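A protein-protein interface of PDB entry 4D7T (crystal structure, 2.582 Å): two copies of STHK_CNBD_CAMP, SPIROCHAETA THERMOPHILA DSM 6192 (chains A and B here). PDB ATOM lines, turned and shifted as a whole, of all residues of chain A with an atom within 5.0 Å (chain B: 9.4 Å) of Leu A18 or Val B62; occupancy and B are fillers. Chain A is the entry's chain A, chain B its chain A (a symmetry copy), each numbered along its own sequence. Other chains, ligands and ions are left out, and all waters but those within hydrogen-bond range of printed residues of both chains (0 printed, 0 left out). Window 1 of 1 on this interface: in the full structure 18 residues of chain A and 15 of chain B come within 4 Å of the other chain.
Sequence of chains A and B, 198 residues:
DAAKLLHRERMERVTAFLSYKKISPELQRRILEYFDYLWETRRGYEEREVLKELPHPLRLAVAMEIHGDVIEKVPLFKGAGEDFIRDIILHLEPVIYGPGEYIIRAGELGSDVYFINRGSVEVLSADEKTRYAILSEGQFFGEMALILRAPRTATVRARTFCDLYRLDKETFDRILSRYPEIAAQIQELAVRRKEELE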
ATOM      1  N   VAL A  14      12.256 -27.251  -2.670  1.00  0.00           N
ATOM      2  CA  VAL A  14      11.772 -25.959  -2.211  1.00  0.00           C
ATOM      3  C   VAL A  14      11.998 -24.905  -3.295  1.00  0.00           C
ATOM      4  O   VAL A  14      11.104 -24.121  -3.597  1.00  0.00           O
ATOM      5  CB  VAL A  14      12.468 -25.516  -0.898  1.00  0.00           C
ATOM      6  CG1 VAL A  14      11.848 -24.235  -0.362  1.00  0.00           C
ATOM      7  CG2 VAL A  14      12.396 -26.617   0.151  1.00  0.00           C
ATOM      8  N   THR A  15      13.187 -24.913  -3.896  1.00  0.00           N
ATOM      9  CA  THR A  15      13.564 -23.931  -4.914  1.00  0.00           C
ATOM     10  C   THR A  15      12.670 -24.020  -6.155  1.00  0.00           C
ATOM     11  O   THR A  15      12.189 -23.000  -6.649  1.00  0.00           O
ATOM     12  CB  THR A  15      15.039 -24.101  -5.335  1.00  0.00           C
ATOM     13  OG1 THR A  15      15.880 -24.065  -4.175  1.00  0.00           O
ATOM     14  CG2 THR A  15      15.457 -23.001  -6.299  1.00  0.00           C
ATOM     15  N   ALA A  16      12.449 -25.233  -6.655  1.00  0.00           N
ATOM     16  CA  ALA A  16      11.559 -25.443  -7.797  1.00  0.00           C
ATOM     17  C   ALA A  16      10.140 -24.956  -7.504  1.00  0.00           C
ATOM     18  O   ALA A  16       9.538 -24.254  -8.315  1.00  0.00           O
ATOM     19  CB  ALA A  16      11.538 -26.911  -8.197  1.00  0.00           C
ATOM     20  N   PHE A  17       9.620 -25.333  -6.341  1.00  0.00           N
ATOM     21  CA  PHE A  17       8.279 -24.938  -5.917  1.00  0.00           C
ATOM     22  C   PHE A  17       8.132 -23.420  -5.834  1.00  0.00           C
ATOM     23  O   PHE A  17       7.133 -22.865  -6.288  1.00  0.00           O
ATOM     24  CB  PHE A  17       7.953 -25.588  -4.567  1.00  0.00           C
ATOM     25  CG  PHE A  17       6.720 -25.040  -3.901  1.00  0.00           C
ATOM     26  CD1 PHE A  17       5.456 -25.381  -4.359  1.00  0.00           C
ATOM     27  CD2 PHE A  17       6.824 -24.205  -2.794  1.00  0.00           C
ATOM     28  CE1 PHE A  17       4.315 -24.887  -3.742  1.00  0.00           C
ATOM     29  CE2 PHE A  17       5.683 -23.707  -2.171  1.00  0.00           C
ATOM     30  CZ  PHE A  17       4.429 -24.049  -2.647  1.00  0.00           C
ATOM     31  N   LEU A  18       9.135 -22.757  -5.265  1.00  0.00           N
ATOM     32  CA  LEU A  18       9.100 -21.309  -5.084  1.00  0.00           C
ATOM     33  C   LEU A  18       9.302 -20.561  -6.401  1.00  0.00           C
ATOM     34  O   LEU A  18       8.773 -19.466  -6.585  1.00  0.00           O
ATOM     35  CB  LEU A  18      10.152 -20.876  -4.061  1.00  0.00           C
ATOM     36  CG  LEU A  18       9.950 -21.382  -2.626  1.00  0.00           C
ATOM     37  CD1 LEU A  18      11.015 -20.838  -1.681  1.00  0.00           C
ATOM     38  CD2 LEU A  18       8.560 -21.034  -2.129  1.00  0.00           C
ATOM     39  N   SER A  19      10.072 -21.152  -7.309  1.00  0.00           N
ATOM     40  CA  SER A  19      10.219 -20.611  -8.655  1.00  0.00           C
ATOM     41  C   SER A  19       8.882 -20.665  -9.390  1.00  0.00           C
ATOM     42  O   SER A  19       8.496 -19.717 -10.073  1.00  0.00           O
ATOM     43  CB  SER A  19      11.292 -21.381  -9.424  1.00  0.00           C
ATOM     44  OG  SER A  19      11.431 -20.905 -10.751  1.00  0.00           O
ATOM     45  N   TYR A  20       8.182 -21.783  -9.221  1.00  0.00           N
ATOM     46  CA  TYR A  20       6.860 -21.995  -9.798  1.00  0.00           C
ATOM     47  C   TYR A  20       5.815 -21.058  -9.198  1.00  0.00           C
ATOM     48  O   TYR A  20       4.916 -20.596  -9.899  1.00  0.00           O
ATOM     49  CB  TYR A  20       6.452 -23.461  -9.605  1.00  0.00           C
ATOM     50  CG  TYR A  20       4.968 -23.740  -9.660  1.00  0.00           C
ATOM     51  CD1 TYR A  20       4.235 -23.519 -10.815  1.00  0.00           C
ATOM     52  CD2 TYR A  20       4.301 -24.249  -8.556  1.00  0.00           C
ATOM     53  CE1 TYR A  20       2.874 -23.779 -10.864  1.00  0.00           C
ATOM     54  CE2 TYR A  20       2.943 -24.514  -8.596  1.00  0.00           C
ATOM     55  CZ  TYR A  20       2.234 -24.277  -9.751  1.00  0.00           C
ATOM     56  OH  TYR A  20       0.884 -24.540  -9.794  1.00  0.00           O
ATOM     57  N   LYS A  21       5.933 -20.777  -7.903  1.00  0.00           N
ATOM     58  CA  LYS A  21       5.008 -19.872  -7.233  1.00  0.00           C
ATOM     59  C   LYS A  21       5.382 -18.417  -7.503  1.00  0.00           C
ATOM     60  O   LYS A  21       4.746 -17.499  -6.976  1.00  0.00           O
ATOM     61  CB  LYS A  21       4.983 -20.133  -5.727  1.00  0.00           C
ATOM     62  CG  LYS A  21       4.498 -21.511  -5.315  1.00  0.00           C
ATOM     63  CD  LYS A  21       3.173 -21.863  -5.966  1.00  0.00           C
ATOM     64  CE  LYS A  21       2.041 -20.975  -5.479  1.00  0.00           C
ATOM     65  NZ  LYS A  21       0.762 -21.267  -6.187  1.00  0.00           N
ATOM     66  N   LYS A  22       6.424 -18.224  -8.311  1.00  0.00           N
ATOM     67  CA  LYS A  22       6.865 -16.899  -8.746  1.00  0.00           C
ATOM     68  C   LYS A  22       7.138 -15.942  -7.591  1.00  0.00           C
ATOM     69  O   LYS A  22       6.590 -14.839  -7.548  1.00  0.00           O
ATOM     70  CB  LYS A  22       5.832 -16.286  -9.693  1.00  0.00           C
ATOM     71  CG  LYS A  22       5.723 -17.020 -11.014  1.00  0.00           C
ATOM     72  CD  LYS A  22       4.592 -16.479 -11.858  1.00  0.00           C
ATOM     73  CE  LYS A  22       4.795 -16.863 -13.307  1.00  0.00           C
ATOM     74  NZ  LYS A  22       5.596 -18.120 -13.433  1.00  0.00           N
ATOM     75  N   ILE A  23       8.005 -16.360  -6.672  1.00  0.00           N
ATOM     76  CA  ILE A  23       8.430 -15.499  -5.574  1.00  0.00           C
ATOM     77  C   ILE A  23       9.498 -14.523  -6.069  1.00  0.00           C
ATOM     78  O   ILE A  23      10.122 -14.755  -7.101  1.00  0.00           O
ATOM     79  CB  ILE A  23       8.981 -16.314  -4.372  1.00  0.00           C
ATOM     80  CG1 ILE A  23      10.337 -16.940  -4.705  1.00  0.00           C
ATOM     81  CG2 ILE A  23       7.989 -17.387  -3.949  1.00  0.00           C
ATOM     82  CD1 ILE A  23      11.066 -17.480  -3.485  1.00  0.00           C
ATOM     83  N   LEU A  27      13.557 -12.544  -1.861  1.00  0.00           N
ATOM     84  CA  LEU A  27      13.092 -13.627  -1.005  1.00  0.00           C
ATOM     85  C   LEU A  27      13.791 -14.932  -1.368  1.00  0.00           C
ATOM     86  O   LEU A  27      14.287 -15.635  -0.491  1.00  0.00           O
ATOM     87  CB  LEU A  27      11.572 -13.790  -1.107  1.00  0.00           C
ATOM     88  CG  LEU A  27      11.002 -14.992  -0.343  1.00  0.00           C
ATOM     89  CD1 LEU A  27      11.393 -14.915   1.120  1.00  0.00           C
ATOM     90  CD2 LEU A  27       9.483 -15.111  -0.489  1.00  0.00           C
ATOM     91  N   ILE A  31      16.200 -17.479   0.955  1.00  0.00           N
ATOM     92  CA  ILE A  31      16.010 -18.919   1.078  1.00  0.00           C
ATOM     93  C   ILE A  31      17.339 -19.650   0.870  1.00  0.00           C
ATOM     94  O   ILE A  31      17.703 -20.518   1.661  1.00  0.00           O
ATOM     95  CB  ILE A  31      14.956 -19.452   0.067  1.00  0.00           C
ATOM     96  CG1 ILE A  31      13.639 -18.670   0.188  1.00  0.00           C
ATOM     97  CG2 ILE A  31      14.739 -20.956   0.246  1.00  0.00           C
ATOM     98  CD1 ILE A  31      12.941 -18.809   1.534  1.00  0.00           C
ATOM     99  N   TYR B  45       3.124 -30.190  -6.493  1.00  0.00           N
ATOM    100  CA  TYR B  45       3.772 -29.779  -5.256  1.00  0.00           C
ATOM    101  C   TYR B  45       2.798 -29.856  -4.086  1.00  0.00           C
ATOM    102  O   TYR B  45       1.585 -29.756  -4.268  1.00  0.00           O
ATOM    103  CB  TYR B  45       4.327 -28.363  -5.378  1.00  0.00           C
ATOM    104  CG  TYR B  45       5.369 -28.193  -6.458  1.00  0.00           C
ATOM    105  CD1 TYR B  45       6.663 -28.656  -6.284  1.00  0.00           C
ATOM    106  CD2 TYR B  45       5.063 -27.547  -7.642  1.00  0.00           C
ATOM    107  CE1 TYR B  45       7.620 -28.494  -7.272  1.00  0.00           C
ATOM    108  CE2 TYR B  45       6.011 -27.380  -8.632  1.00  0.00           C
ATOM    109  CZ  TYR B  45       7.287 -27.856  -8.443  1.00  0.00           C
ATOM    110  OH  TYR B  45       8.229 -27.688  -9.430  1.00  0.00           O
ATOM    111  N   GLU B  47       2.501 -27.870  -0.676  1.00  0.00           N
ATOM    112  CA  GLU B  47       2.998 -26.729   0.090  1.00  0.00           C
ATOM    113  C   GLU B  47       3.388 -27.073   1.528  1.00  0.00           C
ATOM    114  O   GLU B  47       4.358 -26.533   2.064  1.00  0.00           O
ATOM    115  CB  GLU B  47       1.950 -25.615   0.087  1.00  0.00           C
ATOM    116  CG  GLU B  47       2.312 -24.418   0.944  1.00  0.00           C
ATOM    117  CD  GLU B  47       1.436 -23.224   0.665  1.00  0.00           C
ATOM    118  OE1 GLU B  47       0.728 -23.232  -0.363  1.00  0.00           O
ATOM    119  OE2 GLU B  47       1.457 -22.270   1.470  1.00  0.00           O
ATOM    120  N   VAL B  50       6.715 -29.494   1.377  1.00  0.00           N
ATOM    121  CA  VAL B  50       7.880 -28.845   0.782  1.00  0.00           C
ATOM    122  C   VAL B  50       8.444 -27.738   1.680  1.00  0.00           C
ATOM    123  O   VAL B  50       9.647 -27.467   1.657  1.00  0.00           O
ATOM    124  CB  VAL B  50       7.538 -28.270  -0.621  1.00  0.00           C
ATOM    125  CG1 VAL B  50       6.461 -27.207  -0.522  1.00  0.00           C
ATOM    126  CG2 VAL B  50       8.775 -27.716  -1.310  1.00  0.00           C
ATOM    127  N   LEU B  51       7.587 -27.123   2.491  1.00  0.00           N
ATOM    128  CA  LEU B  51       7.999 -25.987   3.308  1.00  0.00           C
ATOM    129  C   LEU B  51       8.119 -26.331   4.796  1.00  0.00           C
ATOM    130  O   LEU B  51       8.398 -25.455   5.614  1.00  0.00           O
ATOM    131  CB  LEU B  51       7.013 -24.826   3.122  1.00  0.00           C
ATOM    132  CG  LEU B  51       6.787 -24.340   1.682  1.00  0.00           C
ATOM    133  CD1 LEU B  51       5.719 -23.251   1.617  1.00  0.00           C
ATOM    134  CD2 LEU B  51       8.086 -23.853   1.070  1.00  0.00           C
ATOM    135  N   LEU B  54      11.170 -25.399   7.066  1.00  0.00           N
ATOM    136  CA  LEU B  54      11.535 -23.986   7.019  1.00  0.00           C
ATOM    137  C   LEU B  54      11.320 -23.324   8.375  1.00  0.00           C
ATOM    138  O   LEU B  54      10.378 -23.669   9.097  1.00  0.00           O
ATOM    139  CB  LEU B  54      10.736 -23.244   5.943  1.00  0.00           C
ATOM    140  CG  LEU B  54      11.292 -23.169   4.515  1.00  0.00           C
ATOM    141  CD1 LEU B  54      11.364 -24.547   3.872  1.00  0.00           C
ATOM    142  CD2 LEU B  54      10.469 -22.211   3.656  1.00  0.00           C
ATOM    143  N   PRO B  55      12.208 -22.382   8.737  1.00  0.00           N
ATOM    144  CA  PRO B  55      12.007 -21.570   9.943  1.00  0.00           C
ATOM    145  C   PRO B  55      10.740 -20.724   9.829  1.00  0.00           C
ATOM    146  O   PRO B  55      10.354 -20.383   8.713  1.00  0.00           O
ATOM    147  CB  PRO B  55      13.255 -20.681   9.991  1.00  0.00           C
ATOM    148  CG  PRO B  55      14.281 -21.418   9.208  1.00  0.00           C
ATOM    149  CD  PRO B  55      13.517 -22.120   8.113  1.00  0.00           C
ATOM    150  N   HIS B  56      10.116 -20.389  10.955  1.00  0.00           N
ATOM    151  CA  HIS B  56       8.885 -19.595  10.960  1.00  0.00           C
ATOM    152  C   HIS B  56       8.971 -18.268  10.180  1.00  0.00           C
ATOM    153  O   HIS B  56       8.077 -17.976   9.383  1.00  0.00           O
ATOM    154  CB  HIS B  56       8.459 -19.323  12.410  1.00  0.00           C
ATOM    155  CG  HIS B  56       7.206 -18.514  12.539  1.00  0.00           C
ATOM    156  ND1 HIS B  56       5.946 -19.056  12.394  1.00  0.00           N
ATOM    157  CD2 HIS B  56       7.021 -17.202  12.816  1.00  0.00           C
ATOM    158  CE1 HIS B  56       5.041 -18.111  12.568  1.00  0.00           C
ATOM    159  NE2 HIS B  56       5.665 -16.975  12.821  1.00  0.00           N
ATOM    160  N   PRO B  57      10.037 -17.464  10.397  1.00  0.00           N
ATOM    161  CA  PRO B  57      10.045 -16.177   9.688  1.00  0.00           C
ATOM    162  C   PRO B  57      10.223 -16.300   8.168  1.00  0.00           C
ATOM    163  O   PRO B  57       9.991 -15.312   7.468  1.00  0.00           O
ATOM    164  CB  PRO B  57      11.236 -15.434  10.318  1.00  0.00           C
ATOM    165  CG  PRO B  57      12.131 -16.516  10.854  1.00  0.00           C
ATOM    166  CD  PRO B  57      11.195 -17.603  11.304  1.00  0.00           C
ATOM    167  N   LEU B  58      10.645 -17.466   7.677  1.00  0.00           N
ATOM    168  CA  LEU B  58      10.708 -17.715   6.238  1.00  0.00           C
ATOM    169  C   LEU B  58       9.361 -18.219   5.727  1.00  0.00           C
ATOM    170  O   LEU B  58       8.902 -17.807   4.661  1.00  0.00           O
ATOM    171  CB  LEU B  58      11.807 -18.723   5.896  1.00  0.00           C
ATOM    172  CG  LEU B  58      13.251 -18.219   5.770  1.00  0.00           C
ATOM    173  CD1 LEU B  58      14.166 -19.309   5.229  1.00  0.00           C
ATOM    174  CD2 LEU B  58      13.314 -16.980   4.897  1.00  0.00           C
ATOM    175  N   ARG B  59       8.738 -19.111   6.494  1.00  0.00           N
ATOM    176  CA  ARG B  59       7.381 -19.568   6.216  1.00  0.00           C
ATOM    177  C   ARG B  59       6.442 -18.374   6.109  1.00  0.00           C
ATOM    178  O   ARG B  59       5.474 -18.396   5.349  1.00  0.00           O
ATOM    179  CB  ARG B  59       6.894 -20.521   7.308  1.00  0.00           C
ATOM    180  CG  ARG B  59       7.553 -21.883   7.301  1.00  0.00           C
ATOM    181  CD  ARG B  59       7.314 -22.573   5.972  1.00  0.00           C
ATOM    182  NE  ARG B  59       5.893 -22.719   5.673  1.00  0.00           N
ATOM    183  CZ  ARG B  59       5.181 -23.815   5.924  1.00  0.00           C
ATOM    184  NH1 ARG B  59       5.754 -24.876   6.472  1.00  0.00           N
ATOM    185  NH2 ARG B  59       3.892 -23.854   5.621  1.00  0.00           N
ATOM    186  N   LEU B  60       6.756 -17.334   6.877  1.00  0.00           N
ATOM    187  CA  LEU B  60       5.970 -16.110   6.924  1.00  0.00           C
ATOM    188  C   LEU B  60       6.212 -15.237   5.691  1.00  0.00           C
ATOM    189  O   LEU B  60       5.278 -14.652   5.149  1.00  0.00           O
ATOM    190  CB  LEU B  60       6.291 -15.334   8.205  1.00  0.00           C
ATOM    191  CG  LEU B  60       5.417 -14.124   8.547  1.00  0.00           C
ATOM    192  CD1 LEU B  60       3.980 -14.564   8.738  1.00  0.00           C
ATOM    193  CD2 LEU B  60       5.929 -13.419   9.798  1.00  0.00           C
ATOM    194  N   ALA B  61       7.462 -15.170   5.245  1.00  0.00           N
ATOM    195  CA  ALA B  61       7.817 -14.379   4.071  1.00  0.00           C
ATOM    196  C   ALA B  61       7.286 -15.001   2.772  1.00  0.00           C
ATOM    197  O   ALA B  61       6.776 -14.292   1.901  1.00  0.00           O
ATOM    198  CB  ALA B  61       9.324 -14.201   3.993  1.00  0.00           C
ATOM    199  N   VAL B  62       7.427 -16.318   2.642  1.00  0.00           N
ATOM    200  CA  VAL B  62       6.901 -17.048   1.491  1.00  0.00           C
ATOM    201  C   VAL B  62       5.380 -16.902   1.389  1.00  0.00           C
ATOM    202  O   VAL B  62       4.845 -16.652   0.308  1.00  0.00           O
ATOM    203  CB  VAL B  62       7.265 -18.548   1.564  1.00  0.00           C
ATOM    204  CG1 VAL B  62       6.573 -19.335   0.464  1.00  0.00           C
ATOM    205  CG2 VAL B  62       8.772 -18.740   1.492  1.00  0.00           C
ATOM    206  N   ALA B  63       4.697 -17.043   2.521  1.00  0.00           N
ATOM    207  CA  ALA B  63       3.238 -16.984   2.565  1.00  0.00           C
ATOM    208  C   ALA B  63       2.675 -15.649   2.073  1.00  0.00           C
ATOM    209  O   ALA B  63       1.657 -15.622   1.386  1.00  0.00           O
ATOM    210  CB  ALA B  63       2.750 -17.266   3.977  1.00  0.00           C
ATOM    211  N   MET B  64       3.336 -14.551   2.434  1.00  0.00           N
ATOM    212  CA  MET B  64       2.894 -13.218   2.042  1.00  0.00           C
ATOM    213  C   MET B  64       3.051 -13.010   0.536  1.00  0.00           C
ATOM    214  O   MET B  64       2.336 -12.206  -0.061  1.00  0.00           O
ATOM    215  CB  MET B  64       3.666 -12.142   2.816  1.00  0.00           C
ATOM    216  CG  MET B  64       3.368 -12.098   4.319  1.00  0.00           C
ATOM    217  SD  MET B  64       4.339 -10.862   5.224  1.00  0.00           S
ATOM    218  CE  MET B  64       3.762 -11.116   6.908  1.00  0.00           C
ATOM    219  N   GLU B  65       3.985 -13.737  -0.074  1.00  0.00           N
ATOM    220  CA  GLU B  65       4.215 -13.630  -1.515  1.00  0.00           C
ATOM    221  C   GLU B  65       3.305 -14.562  -2.311  1.00  0.00           C
ATOM    222  O   GLU B  65       2.691 -14.145  -3.294  1.00  0.00           O
ATOM    223  CB  GLU B  65       5.680 -13.919  -1.862  1.00  0.00           C
ATOM    224  CG  GLU B  65       6.661 -12.838  -1.409  1.00  0.00           C
ATOM    225  CD  GLU B  65       7.848 -12.701  -2.347  1.00  0.00           C
ATOM    226  OE1 GLU B  65       7.759 -13.186  -3.497  1.00  0.00           O
ATOM    227  OE2 GLU B  65       8.862 -12.088  -1.948  1.00  0.00           O
ATOM    228  N   ILE B  66       3.221 -15.822  -1.889  1.00  0.00           N
ATOM    229  CA  ILE B  66       2.490 -16.831  -2.657  1.00  0.00           C
ATOM    230  C   ILE B  66       0.998 -16.875  -2.321  1.00  0.00           C
ATOM    231  O   ILE B  66       0.194 -17.358  -3.122  1.00  0.00           O
ATOM    232  CB  ILE B  66       3.091 -18.247  -2.454  1.00  0.00           C
ATOM    233  CG1 ILE B  66       2.767 -18.801  -1.067  1.00  0.00           C
ATOM    234  CG2 ILE B  66       4.597 -18.224  -2.678  1.00  0.00           C
ATOM    235  CD1 ILE B  66       3.266 -20.241  -0.865  1.00  0.00           C
ATOM    236  N   HIS B  67       0.631 -16.382  -1.141  1.00  0.00           N
ATOM    237  CA  HIS B  67      -0.775 -16.284  -0.765  1.00  0.00           C
ATOM    238  C   HIS B  67      -1.184 -14.823  -0.619  1.00  0.00           C
ATOM    239  O   HIS B  67      -2.118 -14.498   0.116  1.00  0.00           O
ATOM    240  CB  HIS B  67      -1.051 -17.052   0.529  1.00  0.00           C
ATOM    241  CG  HIS B  67      -0.706 -18.506   0.453  1.00  0.00           C
ATOM    242  ND1 HIS B  67      -1.165 -19.327  -0.560  1.00  0.00           N
ATOM    243  CD2 HIS B  67       0.040 -19.287   1.260  1.00  0.00           C
ATOM    244  CE1 HIS B  67      -0.706 -20.548  -0.371  1.00  0.00           C
ATOM    245  NE2 HIS B  67       0.027 -20.557   0.726  1.00  0.00           N
ATOM    246  N   GLY B  68      -0.480 -13.946  -1.331  1.00  0.00           N
ATOM    247  CA  GLY B  68      -0.804 -12.532  -1.339  1.00  0.00           C
ATOM    248  C   GLY B  68      -2.009 -12.210  -2.201  1.00  0.00           C
ATOM    249  O   GLY B  68      -2.734 -11.257  -1.910  1.00  0.00           O
ATOM    250  N   ASP B  69      -2.220 -13.007  -3.251  1.00  0.00           N
ATOM    251  CA  ASP B  69      -3.334 -12.808  -4.180  1.00  0.00           C
ATOM    252  C   ASP B  69      -4.677 -12.643  -3.467  1.00  0.00           C
ATOM    253  O   ASP B  69      -5.433 -11.722  -3.780  1.00  0.00           O
ATOM    254  CB  ASP B  69      -3.410 -13.965  -5.177  1.00  0.00           C
ATOM    255  CG  ASP B  69      -3.184 -15.313  -4.527  1.00  0.00           C
ATOM    256  OD1 ASP B  69      -3.183 -15.385  -3.279  1.00  0.00           O
ATOM    257  OD2 ASP B  69      -3.032 -16.309  -5.263  1.00  0.00           O
ATOM    258  N   ILE B  89      -1.800 -14.584   7.694  1.00  0.00           N
ATOM    259  CA  ILE B  89      -1.377 -15.217   6.450  1.00  0.00           C
ATOM    260  C   ILE B  89      -1.025 -16.700   6.637  1.00  0.00           C
ATOM    261  O   ILE B  89      -1.153 -17.488   5.699  1.00  0.00           O
ATOM    262  CB  ILE B  89      -0.184 -14.452   5.815  1.00  0.00           C
ATOM    263  CG1 ILE B  89      -0.121 -14.692   4.305  1.00  0.00           C
ATOM    264  CG2 ILE B  89       1.132 -14.819   6.482  1.00  0.00           C
ATOM    265  CD1 ILE B  89      -1.334 -14.179   3.570  1.00  0.00           C
ATOM    266  N   LEU B  90      -0.625 -17.079   7.847  1.00  0.00           N
ATOM    267  CA  LEU B  90      -0.271 -18.463   8.138  1.00  0.00           C
ATOM    268  C   LEU B  90      -1.466 -19.245   8.685  1.00  0.00           C
ATOM    269  O   LEU B  90      -1.355 -20.442   8.949  1.00  0.00           O
ATOM    270  CB  LEU B  90       0.899 -18.518   9.125  1.00  0.00           C
ATOM    271  CG  LEU B  90       2.251 -18.024   8.594  1.00  0.00           C
ATOM    272  CD1 LEU B  90       3.339 -18.148   9.648  1.00  0.00           C
ATOM    273  CD2 LEU B  90       2.632 -18.793   7.346  1.00  0.00           C
ATOM    274  N   TYR B 165      -9.735 -20.301   1.060  1.00  0.00           N
ATOM    275  CA  TYR B 165      -8.831 -20.244   2.194  1.00  0.00           C
ATOM    276  C   TYR B 165      -9.663 -20.293   3.465  1.00  0.00           C
ATOM    277  O   TYR B 165     -10.550 -19.457   3.663  1.00  0.00           O
ATOM    278  CB  TYR B 165      -7.956 -18.990   2.129  1.00  0.00           C
ATOM    279  CG  TYR B 165      -6.834 -19.122   1.127  1.00  0.00           C
ATOM    280  CD1 TYR B 165      -7.083 -19.059  -0.229  1.00  0.00           C
ATOM    281  CD2 TYR B 165      -5.533 -19.341   1.538  1.00  0.00           C
ATOM    282  CE1 TYR B 165      -6.065 -19.199  -1.153  1.00  0.00           C
ATOM    283  CE2 TYR B 165      -4.505 -19.474   0.618  1.00  0.00           C
ATOM    284  CZ  TYR B 165      -4.778 -19.400  -0.725  1.00  0.00           C
ATOM    285  OH  TYR B 165      -3.760 -19.535  -1.636  1.00  0.00           O
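Hydrophobic or aromatic side chains of chain A within 4 Å of the printed part of chain B: Val A14, Ala A16, Phe A17, Leu A18, Tyr A20, Ile A23, Leu A27 and Ile A31.
Hydrophobic or aromatic side chains of chain B that line the printed part of chain A: Tyr B45, Val B50, Leu B51, Leu B58, Ala B61, Val B62 and Ile B66.
Among the printed residues, 14 pairs touch across the chains.
O of Leu A18 sits at hydrogen-bond distance from N of Ile A23, 3.2 Å away.
The backbone carbonyl oxygen of Leu B51 lies within hydrogen-bond range of the guanidinium group of Arg B59, at 2.8 Å.
Printed residues of chain B within 4 Å of Leu A18: Val B62 (3.7 Å).
Of chain A, only Leu A18 (3.7 Å) and Leu A27 (3.8 Å) come within 4 Å of Val B62.
Ile A23 touches just these residues of chain B: Glu B65 (3.2 Å) and Ile B66 (3.7 Å).
Of the printed residues of chain B, Ile A31 touches Leu B58.
Of the printed residues of chain B, Phe A17 touches Tyr B45 (3.3 Å), Val B50 (3.8 Å) and Leu B51 (3.8 Å).
Of the printed residues of chain A, Glu B65 touches Ile A23 and Leu A27.
Of the printed residues of chain B, Val A14 touches Val B50.
Ile B89 touches none of the printed residues of chain A.
Gly B68 touches none of the printed residues of chain A.
Val B50 touches Val A14 (O to CG2, 3.2 Å).
Tyr B45 touches Ala A16 (OH to CB, 3.6 Å).
Phe A17 touches Tyr B45.
CG1 of Val B50 touches CD2 of Phe A17 (3.8 Å).
Leu B51 touches Phe A17 (CD1 to CE2, 3.8 Å).
Glu B65 touches Ile A23.
Ile A23 touches Ile B66 (CG2 to CG2, 3.7 Å).
CB of Ala B61 touches CD1 of Leu A27, at 3.6 Å.
Leu A27 touches Val B62.
Ile A31 touches Leu B58 (CD1 to CD2, 3.8 Å).
No position is printed for both chains.
Of the 14 pairs that touch across the chains among the printed residues, none has its exchanged pair printed and touching as well.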
